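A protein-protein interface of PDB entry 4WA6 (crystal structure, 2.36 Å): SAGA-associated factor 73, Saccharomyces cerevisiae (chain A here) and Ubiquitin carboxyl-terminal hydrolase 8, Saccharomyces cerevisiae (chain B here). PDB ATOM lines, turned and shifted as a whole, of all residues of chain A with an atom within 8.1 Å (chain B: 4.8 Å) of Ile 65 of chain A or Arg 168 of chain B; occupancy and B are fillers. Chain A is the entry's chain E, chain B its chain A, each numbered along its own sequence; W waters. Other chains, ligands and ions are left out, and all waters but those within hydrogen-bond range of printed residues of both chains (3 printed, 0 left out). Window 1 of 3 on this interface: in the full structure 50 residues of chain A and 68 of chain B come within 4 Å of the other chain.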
ATOM      1  N   LEU A  44     -18.484   6.740  11.002  1.00  0.00           N
ATOM      2  CA  LEU A  44     -17.768   7.943  11.207  1.00  0.00           C
ATOM      3  C   LEU A  44     -17.708   8.220  12.716  1.00  0.00           C
ATOM      4  O   LEU A  44     -18.729   8.212  13.408  1.00  0.00           O
ATOM      5  CB  LEU A  44     -18.469   9.049  10.435  1.00  0.00           C
ATOM      6  CG  LEU A  44     -18.015  10.445  10.803  1.00  0.00           C
ATOM      7  CD1 LEU A  44     -16.555  10.677  10.419  1.00  0.00           C
ATOM      8  CD2 LEU A  44     -18.961  11.435  10.143  1.00  0.00           C
ATOM      9  N   TYR A  46     -16.465  10.549  16.069  1.00  0.00           N
ATOM     10  CA  TYR A  46     -16.143  11.887  16.551  1.00  0.00           C
ATOM     11  C   TYR A  46     -15.190  11.781  17.689  1.00  0.00           C
ATOM     12  O   TYR A  46     -15.089  10.769  18.344  1.00  0.00           O
ATOM     13  CB  TYR A  46     -17.406  12.635  16.990  1.00  0.00           C
ATOM     14  CG  TYR A  46     -18.430  12.589  15.890  1.00  0.00           C
ATOM     15  CD1 TYR A  46     -18.329  13.446  14.793  1.00  0.00           C
ATOM     16  CD2 TYR A  46     -19.466  11.646  15.908  1.00  0.00           C
ATOM     17  CE1 TYR A  46     -19.251  13.394  13.766  1.00  0.00           C
ATOM     18  CE2 TYR A  46     -20.401  11.586  14.889  1.00  0.00           C
ATOM     19  CZ  TYR A  46     -20.275  12.455  13.820  1.00  0.00           C
ATOM     20  OH  TYR A  46     -21.163  12.417  12.791  1.00  0.00           O
ATOM     21  N   HIS A  48     -15.062  14.017  20.324  1.00  0.00           N
ATOM     22  CA  HIS A  48     -15.592  14.450  21.606  1.00  0.00           C
ATOM     23  C   HIS A  48     -17.094  14.589  21.548  1.00  0.00           C
ATOM     24  O   HIS A  48     -17.664  15.552  22.042  1.00  0.00           O
ATOM     25  CB  HIS A  48     -14.900  15.761  22.080  1.00  0.00           C
ATOM     26  CG  HIS A  48     -14.820  16.842  21.039  1.00  0.00           C
ATOM     27  ND1 HIS A  48     -13.659  17.116  20.339  1.00  0.00           N
ATOM     28  CD2 HIS A  48     -15.740  17.739  20.604  1.00  0.00           C
ATOM     29  CE1 HIS A  48     -13.878  18.118  19.504  1.00  0.00           C
ATOM     30  NE2 HIS A  48     -15.133  18.513  19.642  1.00  0.00           N
ATOM     31  N   MET A  49     -17.736  13.607  20.942  1.00  0.00           N
ATOM     32  CA  MET A  49     -19.173  13.567  20.891  1.00  0.00           C
ATOM     33  C   MET A  49     -19.492  12.125  21.038  1.00  0.00           C
ATOM     34  O   MET A  49     -19.409  11.385  20.085  1.00  0.00           O
ATOM     35  CB  MET A  49     -19.710  14.175  19.585  1.00  0.00           C
ATOM     36  CG  MET A  49     -19.590  15.690  19.584  1.00  0.00           C
ATOM     37  SD  MET A  49     -20.488  16.687  18.369  1.00  0.00           S
ATOM     38  CE  MET A  49     -20.227  15.701  16.907  1.00  0.00           C
ATOM     39  N   ALA A  62     -29.321  13.414  12.727  1.00  0.00           N
ATOM     40  CA  ALA A  62     -28.708  14.716  12.881  1.00  0.00           C
ATOM     41  C   ALA A  62     -27.472  14.775  12.026  1.00  0.00           C
ATOM     42  O   ALA A  62     -26.745  13.828  11.984  1.00  0.00           O
ATOM     43  CB  ALA A  62     -28.342  14.975  14.328  1.00  0.00           C
ATOM     44  N   GLN A  63     -27.232  15.898  11.361  1.00  0.00           N
ATOM     45  CA  GLN A  63     -25.909  16.229  10.862  1.00  0.00           C
ATOM     46  C   GLN A  63     -25.102  16.737  12.022  1.00  0.00           C
ATOM     47  O   GLN A  63     -25.630  17.458  12.837  1.00  0.00           O
ATOM     48  CB  GLN A  63     -25.982  17.355   9.852  1.00  0.00           C
ATOM     49  CG  GLN A  63     -26.727  17.007   8.577  1.00  0.00           C
ATOM     50  CD  GLN A  63     -26.509  18.036   7.475  1.00  0.00           C
ATOM     51  OE1 GLN A  63     -25.470  18.706   7.415  1.00  0.00           O
ATOM     52  NE2 GLN A  63     -27.496  18.182   6.608  1.00  0.00           N
ATOM     53  N   LEU A  64     -23.826  16.355  12.092  1.00  0.00           N
ATOM     54  CA  LEU A  64     -22.877  16.846  13.093  1.00  0.00           C
ATOM     55  C   LEU A  64     -21.575  17.262  12.414  1.00  0.00           C
ATOM     56  O   LEU A  64     -20.952  16.491  11.734  1.00  0.00           O
ATOM     57  CB  LEU A  64     -22.610  15.754  14.147  1.00  0.00           C
ATOM     58  CG  LEU A  64     -23.862  15.296  14.931  1.00  0.00           C
ATOM     59  CD1 LEU A  64     -23.870  13.804  15.243  1.00  0.00           C
ATOM     60  CD2 LEU A  64     -24.118  16.119  16.201  1.00  0.00           C
ATOM     61  N   ILE A  65     -21.155  18.498  12.578  1.00  0.00           N
ATOM     62  CA  ILE A  65     -19.796  18.896  12.195  1.00  0.00           C
ATOM     63  C   ILE A  65     -19.086  19.230  13.494  1.00  0.00           C
ATOM     64  O   ILE A  65     -19.429  20.173  14.191  1.00  0.00           O
ATOM     65  CB  ILE A  65     -19.801  20.108  11.290  1.00  0.00           C
ATOM     66  CG1 ILE A  65     -20.563  19.844  10.009  1.00  0.00           C
ATOM     67  CG2 ILE A  65     -18.369  20.501  10.937  1.00  0.00           C
ATOM     68  CD1 ILE A  65     -20.778  21.107   9.184  1.00  0.00           C
ATOM     69  N   GLU A  66     -18.136  18.411  13.874  1.00  0.00           N
ATOM     70  CA  GLU A  66     -17.416  18.634  15.107  1.00  0.00           C
ATOM     71  C   GLU A  66     -16.366  19.764  14.946  1.00  0.00           C
ATOM     72  O   GLU A  66     -15.639  19.832  13.984  1.00  0.00           O
ATOM     73  CB  GLU A  66     -16.762  17.319  15.515  1.00  0.00           C
ATOM     74  CG  GLU A  66     -15.907  17.372  16.769  1.00  0.00           C
ATOM     75  CD  GLU A  66     -15.559  15.983  17.248  1.00  0.00           C
ATOM     76  OE1 GLU A  66     -15.078  15.157  16.428  1.00  0.00           O
ATOM     77  OE2 GLU A  66     -15.798  15.713  18.436  1.00  0.00           O
ATOM     78  N   ASP A  67     -16.323  20.667  15.895  1.00  0.00           N
ATOM     79  CA  ASP A  67     -15.391  21.777  15.880  1.00  0.00           C
ATOM     80  C   ASP A  67     -15.467  22.513  14.547  1.00  0.00           C
ATOM     81  O   ASP A  67     -14.465  22.744  13.911  1.00  0.00           O
ATOM     82  CB  ASP A  67     -13.971  21.299  16.219  1.00  0.00           C
ATOM     83  CG  ASP A  67     -13.816  20.972  17.687  1.00  0.00           C
ATOM     84  OD1 ASP A  67     -14.813  21.123  18.474  1.00  0.00           O
ATOM     85  OD2 ASP A  67     -12.683  20.579  18.068  1.00  0.00           O
ATOM     86  N   PRO A  68     -16.679  22.914  14.168  1.00  0.00           N
ATOM     87  CA  PRO A  68     -17.008  23.515  12.893  1.00  0.00           C
ATOM     88  C   PRO A  68     -16.241  24.784  12.607  1.00  0.00           C
ATOM     89  O   PRO A  68     -15.934  25.075  11.466  1.00  0.00           O
ATOM     90  CB  PRO A  68     -18.499  23.836  13.042  1.00  0.00           C
ATOM     91  CG  PRO A  68     -18.704  23.967  14.508  1.00  0.00           C
ATOM     92  CD  PRO A  68     -17.842  22.891  15.073  1.00  0.00           C
ATOM     93  N   LEU A  69     -15.905  25.539  13.622  1.00  0.00           N
ATOM     94  CA  LEU A  69     -15.097  26.755  13.409  1.00  0.00           C
ATOM     95  C   LEU A  69     -13.566  26.557  13.486  1.00  0.00           C
ATOM     96  O   LEU A  69     -12.831  27.521  13.553  1.00  0.00           O
ATOM     97  CB  LEU A  69     -15.577  27.858  14.349  1.00  0.00           C
ATOM     98  CG  LEU A  69     -16.622  28.815  13.773  1.00  0.00           C
ATOM     99  CD1 LEU A  69     -17.787  28.157  13.043  1.00  0.00           C
ATOM    100  CD2 LEU A  69     -17.144  29.712  14.871  1.00  0.00           C
ATOM    101  N   ASP A  70     -13.089  25.310  13.439  1.00  0.00           N
ATOM    102  CA  ASP A  70     -11.654  25.019  13.609  1.00  0.00           C
ATOM    103  C   ASP A  70     -10.905  24.861  12.285  1.00  0.00           C
ATOM    104  O   ASP A  70      -9.742  24.491  12.307  1.00  0.00           O
ATOM    105  CB  ASP A  70     -11.423  23.799  14.529  1.00  0.00           C
ATOM    106  CG  ASP A  70     -11.067  24.203  16.007  1.00  0.00           C
ATOM    107  OD1 ASP A  70     -11.389  25.335  16.432  1.00  0.00           O
ATOM    108  OD2 ASP A  70     -10.444  23.391  16.753  1.00  0.00           O
ATOM    109  N   LYS A  71     -11.572  25.110  11.151  1.00  0.00           N
ATOM    110  CA  LYS A  71     -10.922  25.411   9.847  1.00  0.00           C
ATOM    111  C   LYS A  71     -11.957  26.017   8.911  1.00  0.00           C
ATOM    112  O   LYS A  71     -13.140  25.667   9.021  1.00  0.00           O
ATOM    113  CB  LYS A  71     -10.316  24.173   9.176  1.00  0.00           C
ATOM    114  CG  LYS A  71     -11.337  23.125   8.774  1.00  0.00           C
ATOM    115  CD  LYS A  71     -10.742  22.010   7.922  1.00  0.00           C
ATOM    116  CE  LYS A  71     -11.856  21.194   7.279  1.00  0.00           C
ATOM    117  NZ  LYS A  71     -11.446  19.795   6.966  1.00  0.00           N
ATOM    118  N   ILE A  73     -14.279  26.245   5.666  1.00  0.00           N
ATOM    119  CA  ILE A  73     -14.849  25.235   4.815  1.00  0.00           C
ATOM    120  C   ILE A  73     -13.877  25.251   3.692  1.00  0.00           C
ATOM    121  O   ILE A  73     -13.441  26.341   3.287  1.00  0.00           O
ATOM    122  CB  ILE A  73     -16.276  25.613   4.372  1.00  0.00           C
ATOM    123  CG1 ILE A  73     -16.958  24.421   3.673  1.00  0.00           C
ATOM    124  CG2 ILE A  73     -16.279  26.897   3.533  1.00  0.00           C
ATOM    125  CD1 ILE A  73     -18.405  24.259   4.093  1.00  0.00           C
ATOM    126  N   GLN A  74     -13.436  24.076   3.258  1.00  0.00           N
ATOM    127  CA  GLN A  74     -12.464  24.024   2.187  1.00  0.00           C
ATOM    128  C   GLN A  74     -13.258  24.080   0.907  1.00  0.00           C
ATOM    129  O   GLN A  74     -14.148  23.239   0.657  1.00  0.00           O
ATOM    130  CB  GLN A  74     -11.652  22.756   2.218  1.00  0.00           C
ATOM    131  CG  GLN A  74     -10.797  22.575   3.460  1.00  0.00           C
ATOM    132  CD  GLN A  74     -10.287  21.138   3.524  1.00  0.00           C
ATOM    133  OE1 GLN A  74     -10.900  20.270   4.169  1.00  0.00           O
ATOM    134  NE2 GLN A  74      -9.211  20.857   2.791  1.00  0.00           N
ATOM    135  N   PRO A  84     -18.672  28.762  -5.696  1.00  0.00           N
ATOM    136  CA  PRO A  84     -17.845  28.145  -4.686  1.00  0.00           C
ATOM    137  C   PRO A  84     -18.218  26.664  -4.536  1.00  0.00           C
ATOM    138  O   PRO A  84     -19.354  26.357  -4.222  1.00  0.00           O
ATOM    139  CB  PRO A  84     -18.212  28.932  -3.418  1.00  0.00           C
ATOM    140  CG  PRO A  84     -19.663  29.290  -3.647  1.00  0.00           C
ATOM    141  CD  PRO A  84     -19.725  29.606  -5.116  1.00  0.00           C
ATOM    142  N   LEU A  85     -17.256  25.775  -4.738  1.00  0.00           N
ATOM    143  CA  LEU A  85     -17.496  24.345  -4.681  1.00  0.00           C
ATOM    144  C   LEU A  85     -16.741  23.675  -3.522  1.00  0.00           C
ATOM    145  O   LEU A  85     -15.534  23.873  -3.327  1.00  0.00           O
ATOM    146  CB  LEU A  85     -17.079  23.734  -6.000  1.00  0.00           C
ATOM    147  CG  LEU A  85     -17.708  24.396  -7.243  1.00  0.00           C
ATOM    148  CD1 LEU A  85     -17.064  23.825  -8.463  1.00  0.00           C
ATOM    149  CD2 LEU A  85     -19.199  24.203  -7.337  1.00  0.00           C
ATOM    150  N   ALA A  86     -17.460  22.867  -2.754  1.00  0.00           N
ATOM    151  CA  ALA A  86     -16.850  22.089  -1.692  1.00  0.00           C
ATOM    152  C   ALA A  86     -15.959  21.052  -2.310  1.00  0.00           C
ATOM    153  O   ALA A  86     -16.229  20.611  -3.410  1.00  0.00           O
ATOM    154  CB  ALA A  86     -17.921  21.406  -0.854  1.00  0.00           C
ATOM    155  N   THR A  88     -15.590  17.824  -2.048  1.00  0.00           N
ATOM    156  CA  THR A  88     -16.239  16.618  -2.519  1.00  0.00           C
ATOM    157  C   THR A  88     -17.312  16.910  -3.543  1.00  0.00           C
ATOM    158  O   THR A  88     -18.011  15.997  -3.910  1.00  0.00           O
ATOM    159  CB  THR A  88     -16.954  15.860  -1.378  1.00  0.00           C
ATOM    160  OG1 THR A  88     -17.929  16.714  -0.824  1.00  0.00           O
ATOM    161  CG2 THR A  88     -15.998  15.459  -0.226  1.00  0.00           C
ATOM    162  N   ALA A  89     -17.497  18.156  -3.980  1.00  0.00           N
ATOM    163  CA  ALA A  89     -18.472  18.440  -5.088  1.00  0.00           C
ATOM    164  C   ALA A  89     -17.800  18.850  -6.392  1.00  0.00           C
ATOM    165  O   ALA A  89     -18.453  18.981  -7.392  1.00  0.00           O
ATOM    166  CB  ALA A  89     -19.483  19.496  -4.675  1.00  0.00           C
ATOM    167  N   PRO B 164     -22.099  26.965   9.483  1.00  0.00           N
ATOM    168  CA  PRO B 164     -21.339  25.868   8.865  1.00  0.00           C
ATOM    169  C   PRO B 164     -22.154  24.782   8.192  1.00  0.00           C
ATOM    170  O   PRO B 164     -21.755  24.270   7.137  1.00  0.00           O
ATOM    171  CB  PRO B 164     -20.547  25.280  10.042  1.00  0.00           C
ATOM    172  CG  PRO B 164     -21.224  25.809  11.252  1.00  0.00           C
ATOM    173  CD  PRO B 164     -21.681  27.174  10.871  1.00  0.00           C
ATOM    174  N   TYR B 165     -23.289  24.427   8.786  1.00  0.00           N
ATOM    175  CA  TYR B 165     -24.145  23.418   8.203  1.00  0.00           C
ATOM    176  C   TYR B 165     -24.743  23.863   6.867  1.00  0.00           C
ATOM    177  O   TYR B 165     -24.803  23.107   5.896  1.00  0.00           O
ATOM    178  CB  TYR B 165     -25.221  23.020   9.193  1.00  0.00           C
ATOM    179  CG  TYR B 165     -24.641  22.281  10.390  1.00  0.00           C
ATOM    180  CD1 TYR B 165     -24.436  20.925  10.360  1.00  0.00           C
ATOM    181  CD2 TYR B 165     -24.352  22.947  11.546  1.00  0.00           C
ATOM    182  CE1 TYR B 165     -23.901  20.249  11.443  1.00  0.00           C
ATOM    183  CE2 TYR B 165     -23.837  22.285  12.652  1.00  0.00           C
ATOM    184  CZ  TYR B 165     -23.591  20.935  12.569  1.00  0.00           C
ATOM    185  OH  TYR B 165     -23.088  20.299  13.672  1.00  0.00           O
ATOM    186  N   PHE B 166     -25.171  25.106   6.814  1.00  0.00           N
ATOM    187  CA  PHE B 166     -25.787  25.613   5.638  1.00  0.00           C
ATOM    188  C   PHE B 166     -24.782  25.912   4.546  1.00  0.00           C
ATOM    189  O   PHE B 166     -25.060  25.695   3.354  1.00  0.00           O
ATOM    190  CB  PHE B 166     -26.618  26.841   5.934  1.00  0.00           C
ATOM    191  CG  PHE B 166     -27.470  27.218   4.775  1.00  0.00           C
ATOM    192  CD1 PHE B 166     -28.543  26.423   4.431  1.00  0.00           C
ATOM    193  CD2 PHE B 166     -27.105  28.282   3.936  1.00  0.00           C
ATOM    194  CE1 PHE B 166     -29.300  26.725   3.300  1.00  0.00           C
ATOM    195  CE2 PHE B 166     -27.840  28.573   2.811  1.00  0.00           C
ATOM    196  CZ  PHE B 166     -28.960  27.818   2.503  1.00  0.00           C
ATOM    197  N   ILE B 167     -23.609  26.419   4.917  1.00  0.00           N
ATOM    198  CA  ILE B 167     -22.639  26.700   3.882  1.00  0.00           C
ATOM    199  C   ILE B 167     -22.190  25.382   3.203  1.00  0.00           C
ATOM    200  O   ILE B 167     -22.115  25.328   1.975  1.00  0.00           O
ATOM    201  CB  ILE B 167     -21.417  27.456   4.399  1.00  0.00           C
ATOM    202  CG1 ILE B 167     -21.798  28.764   5.074  1.00  0.00           C
ATOM    203  CG2 ILE B 167     -20.555  27.862   3.236  1.00  0.00           C
ATOM    204  CD1 ILE B 167     -20.725  29.144   6.093  1.00  0.00           C
ATOM    205  N   ARG B 168     -21.928  24.339   4.011  1.00  0.00           N
ATOM    206  CA  ARG B 168     -21.522  23.023   3.505  1.00  0.00           C
ATOM    207  C   ARG B 168     -22.594  22.453   2.618  1.00  0.00           C
ATOM    208  O   ARG B 168     -22.318  21.804   1.608  1.00  0.00           O
ATOM    209  CB  ARG B 168     -21.227  22.032   4.657  1.00  0.00           C
ATOM    210  CG  ARG B 168     -20.885  20.605   4.230  1.00  0.00           C
ATOM    211  CD  ARG B 168     -20.689  19.624   5.391  1.00  0.00           C
ATOM    212  NE  ARG B 168     -21.900  19.164   6.111  1.00  0.00           N
ATOM    213  CZ  ARG B 168     -21.917  18.156   7.004  1.00  0.00           C
ATOM    214  NH1 ARG B 168     -20.802  17.477   7.326  1.00  0.00           N
ATOM    215  NH2 ARG B 168     -23.046  17.798   7.580  1.00  0.00           N
ATOM    216  N   HIS B 169     -23.833  22.709   2.981  1.00  0.00           N
ATOM    217  CA  HIS B 169     -24.937  22.190   2.208  1.00  0.00           C
ATOM    218  C   HIS B 169     -25.034  22.870   0.855  1.00  0.00           C
ATOM    219  O   HIS B 169     -25.182  22.222  -0.164  1.00  0.00           O
ATOM    220  CB  HIS B 169     -26.225  22.443   2.956  1.00  0.00           C
ATOM    221  CG  HIS B 169     -27.410  21.832   2.298  1.00  0.00           C
ATOM    222  ND1 HIS B 169     -28.414  22.581   1.721  1.00  0.00           N
ATOM    223  CD2 HIS B 169     -27.750  20.538   2.120  1.00  0.00           C
ATOM    224  CE1 HIS B 169     -29.332  21.772   1.222  1.00  0.00           C
ATOM    225  NE2 HIS B 169     -28.942  20.525   1.444  1.00  0.00           N
ATOM    226  N   SER B 170     -25.019  24.191   0.869  1.00  0.00           N
ATOM    227  CA  SER B 170     -25.140  24.961  -0.331  1.00  0.00           C
ATOM    228  C   SER B 170     -23.962  24.690  -1.273  1.00  0.00           C
ATOM    229  O   SER B 170     -24.204  24.427  -2.438  1.00  0.00           O
ATOM    230  CB  SER B 170     -25.208  26.429  -0.005  1.00  0.00           C
ATOM    231  OG  SER B 170     -25.429  27.141  -1.203  1.00  0.00           O
ATOM    232  N   MET B 171     -22.710  24.735  -0.769  1.00  0.00           N
ATOM    233  CA  MET B 171     -21.498  24.513  -1.577  1.00  0.00           C
ATOM    234  C   MET B 171     -21.296  23.077  -2.040  1.00  0.00           C
ATOM    235  O   MET B 171     -20.554  22.861  -3.008  1.00  0.00           O
ATOM    236  CB  MET B 171     -20.211  24.912  -0.831  1.00  0.00           C
ATOM    237  CG  MET B 171     -20.084  26.395  -0.571  1.00  0.00           C
ATOM    238  SD  MET B 171     -18.434  26.838  -0.023  1.00  0.00           S
ATOM    239  CE  MET B 171     -18.679  28.575   0.388  1.00  0.00           C
ATOM    240  N   SER B 172     -21.938  22.110  -1.372  1.00  0.00           N
ATOM    241  CA  SER B 172     -21.978  20.722  -1.848  1.00  0.00           C
ATOM    242  C   SER B 172     -22.922  20.553  -3.058  1.00  0.00           C
ATOM    243  O   SER B 172     -23.004  19.476  -3.598  1.00  0.00           O
ATOM    244  CB  SER B 172     -22.524  19.816  -0.769  1.00  0.00           C
ATOM    245  OG  SER B 172     -23.940  19.723  -0.927  1.00  0.00           O
ATOM    246  N   ILE B 472     -23.522  22.662  17.959  1.00  0.00           N
ATOM    247  CA  ILE B 472     -23.154  21.604  18.914  1.00  0.00           C
ATOM    248  C   ILE B 472     -21.624  21.387  18.877  1.00  0.00           C
ATOM    249  O   ILE B 472     -20.989  21.311  17.818  1.00  0.00           O
ATOM    250  CB  ILE B 472     -23.949  20.296  18.688  1.00  0.00           C
ATOM    251  CG1 ILE B 472     -23.771  19.262  19.822  1.00  0.00           C
ATOM    252  CG2 ILE B 472     -23.538  19.654  17.376  1.00  0.00           C
ATOM    253  CD1 ILE B 472     -23.944  19.755  21.263  1.00  0.00           C
HETATM  254  O   HOH W   1     -24.302  20.555   5.833  1.00  0.00           O
HETATM  255  O   HOH W   2     -21.630  21.633  15.112  1.00  0.00           O
HETATM  256  O   HOH W   3     -18.073  20.018  17.766  1.00  0.00           O
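The guanidinium group (NH2) of Arg 168 of chain B is in hydrogen-bond range of the side-chain amide oxygen (OE1) of Gln 63 of chain A (2.6 Å).
O of Met 171 of chain B sits at hydrogen-bond distance from N of Ala 86 of chain A.
N of Ile 65 of chain A is in hydrogen-bond range of OH of Tyr 165 of chain B, at 2.9 Å.
The side-chain hydroxyl (OG) of Ser 172 of chain B lies within hydrogen-bond range of the backbone carbonyl oxygen (O) of His 169 of chain B (2.9 Å).
Among the printed residues, pairs that only touch across the chains: Ile 73 of chain A with Arg 168 of chain B, Leu 64 of chain A with Tyr 165 of chain B, Gln 63 of chain A with Tyr 165 of chain B, Ile 65 of chain A with Arg 168 of chain B, Ala 89 of chain A with Ser 172 of chain B, Pro 84 of chain A with Met 171 of chain B, Leu 64 of chain A with Ile 472 of chain B, Leu 85 of chain A with Met 171 of chain B, Pro 68 of chain A with Pro 164 of chain B, Ile 65 of chain A with Pro 164 of chain B and Ala 89 of chain A with Met 171 of chain B.
Ile 65 of chain A touches just these residues of chain B: Pro 164 (3.9 Å), Tyr 165 (2.9 Å) and Arg 168 (3.6 Å).
Of chain A, only Gln 63, Ile 65 and Ile 73 come within 4 Å of Arg 168 of chain B.
Of the printed residues of chain A, Pro 164 of chain B touches Ile 65 (3.9 Å) and Pro 68 (3.8 Å).
Of the printed residues of chain B, Leu 85 of chain A touches Met 171.
Printed residues of chain A within 4 Å of Met 171 of chain B: Pro 84 (3.7 Å), Leu 85 (3.8 Å), Ala 86 (3.1 Å) and Ala 89 (3.9 Å).
Of the printed residues of chain B, Ile 73 of chain A touches Arg 168.
Phe 166 of chain B touches none of the printed residues of chain A.
The nearest residue of chain A that does not touch Arg 168 of chain B is Leu 64 of chain A (4.5 Å).
Of the 10 printed residues of chain B, 6 touch a printed residue of chain A.
Hydrophobic or aromatic side chains of chain B within 4 Å of the printed part of chain A: Pro 164, Tyr 165, Met 171 and Ile 472.
Along chain A the printed residues that touch a printed residue of chain B span positions 63 to 89.
Among the printed residues, no Asp or Glu carboxylate lies within 4 Å of a Lys or Arg side-chain nitrogen of the other chain.
Water W2 lies within hydrogen-bond range of the side-chain hydroxyl of Tyr 165 of chain B, the backbone carbonyl oxygen of Ile 65 of chain A and the backbone carbonyl oxygen of Ile 472 of chain B.
Water W1 lies within hydrogen-bond range of the backbone carbonyl oxygen of Tyr 165 of chain B (2.6 Å), the side-chain amide oxygen of Gln 63 of chain A (2.7 Å) and the guanidinium group of Arg 168 of chain B (2.8 Å).
Water W3 lies within hydrogen-bond range of N of Asp 67 of chain A (2.6 Å) and O of Ile 472 of chain B (3.2 Å).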
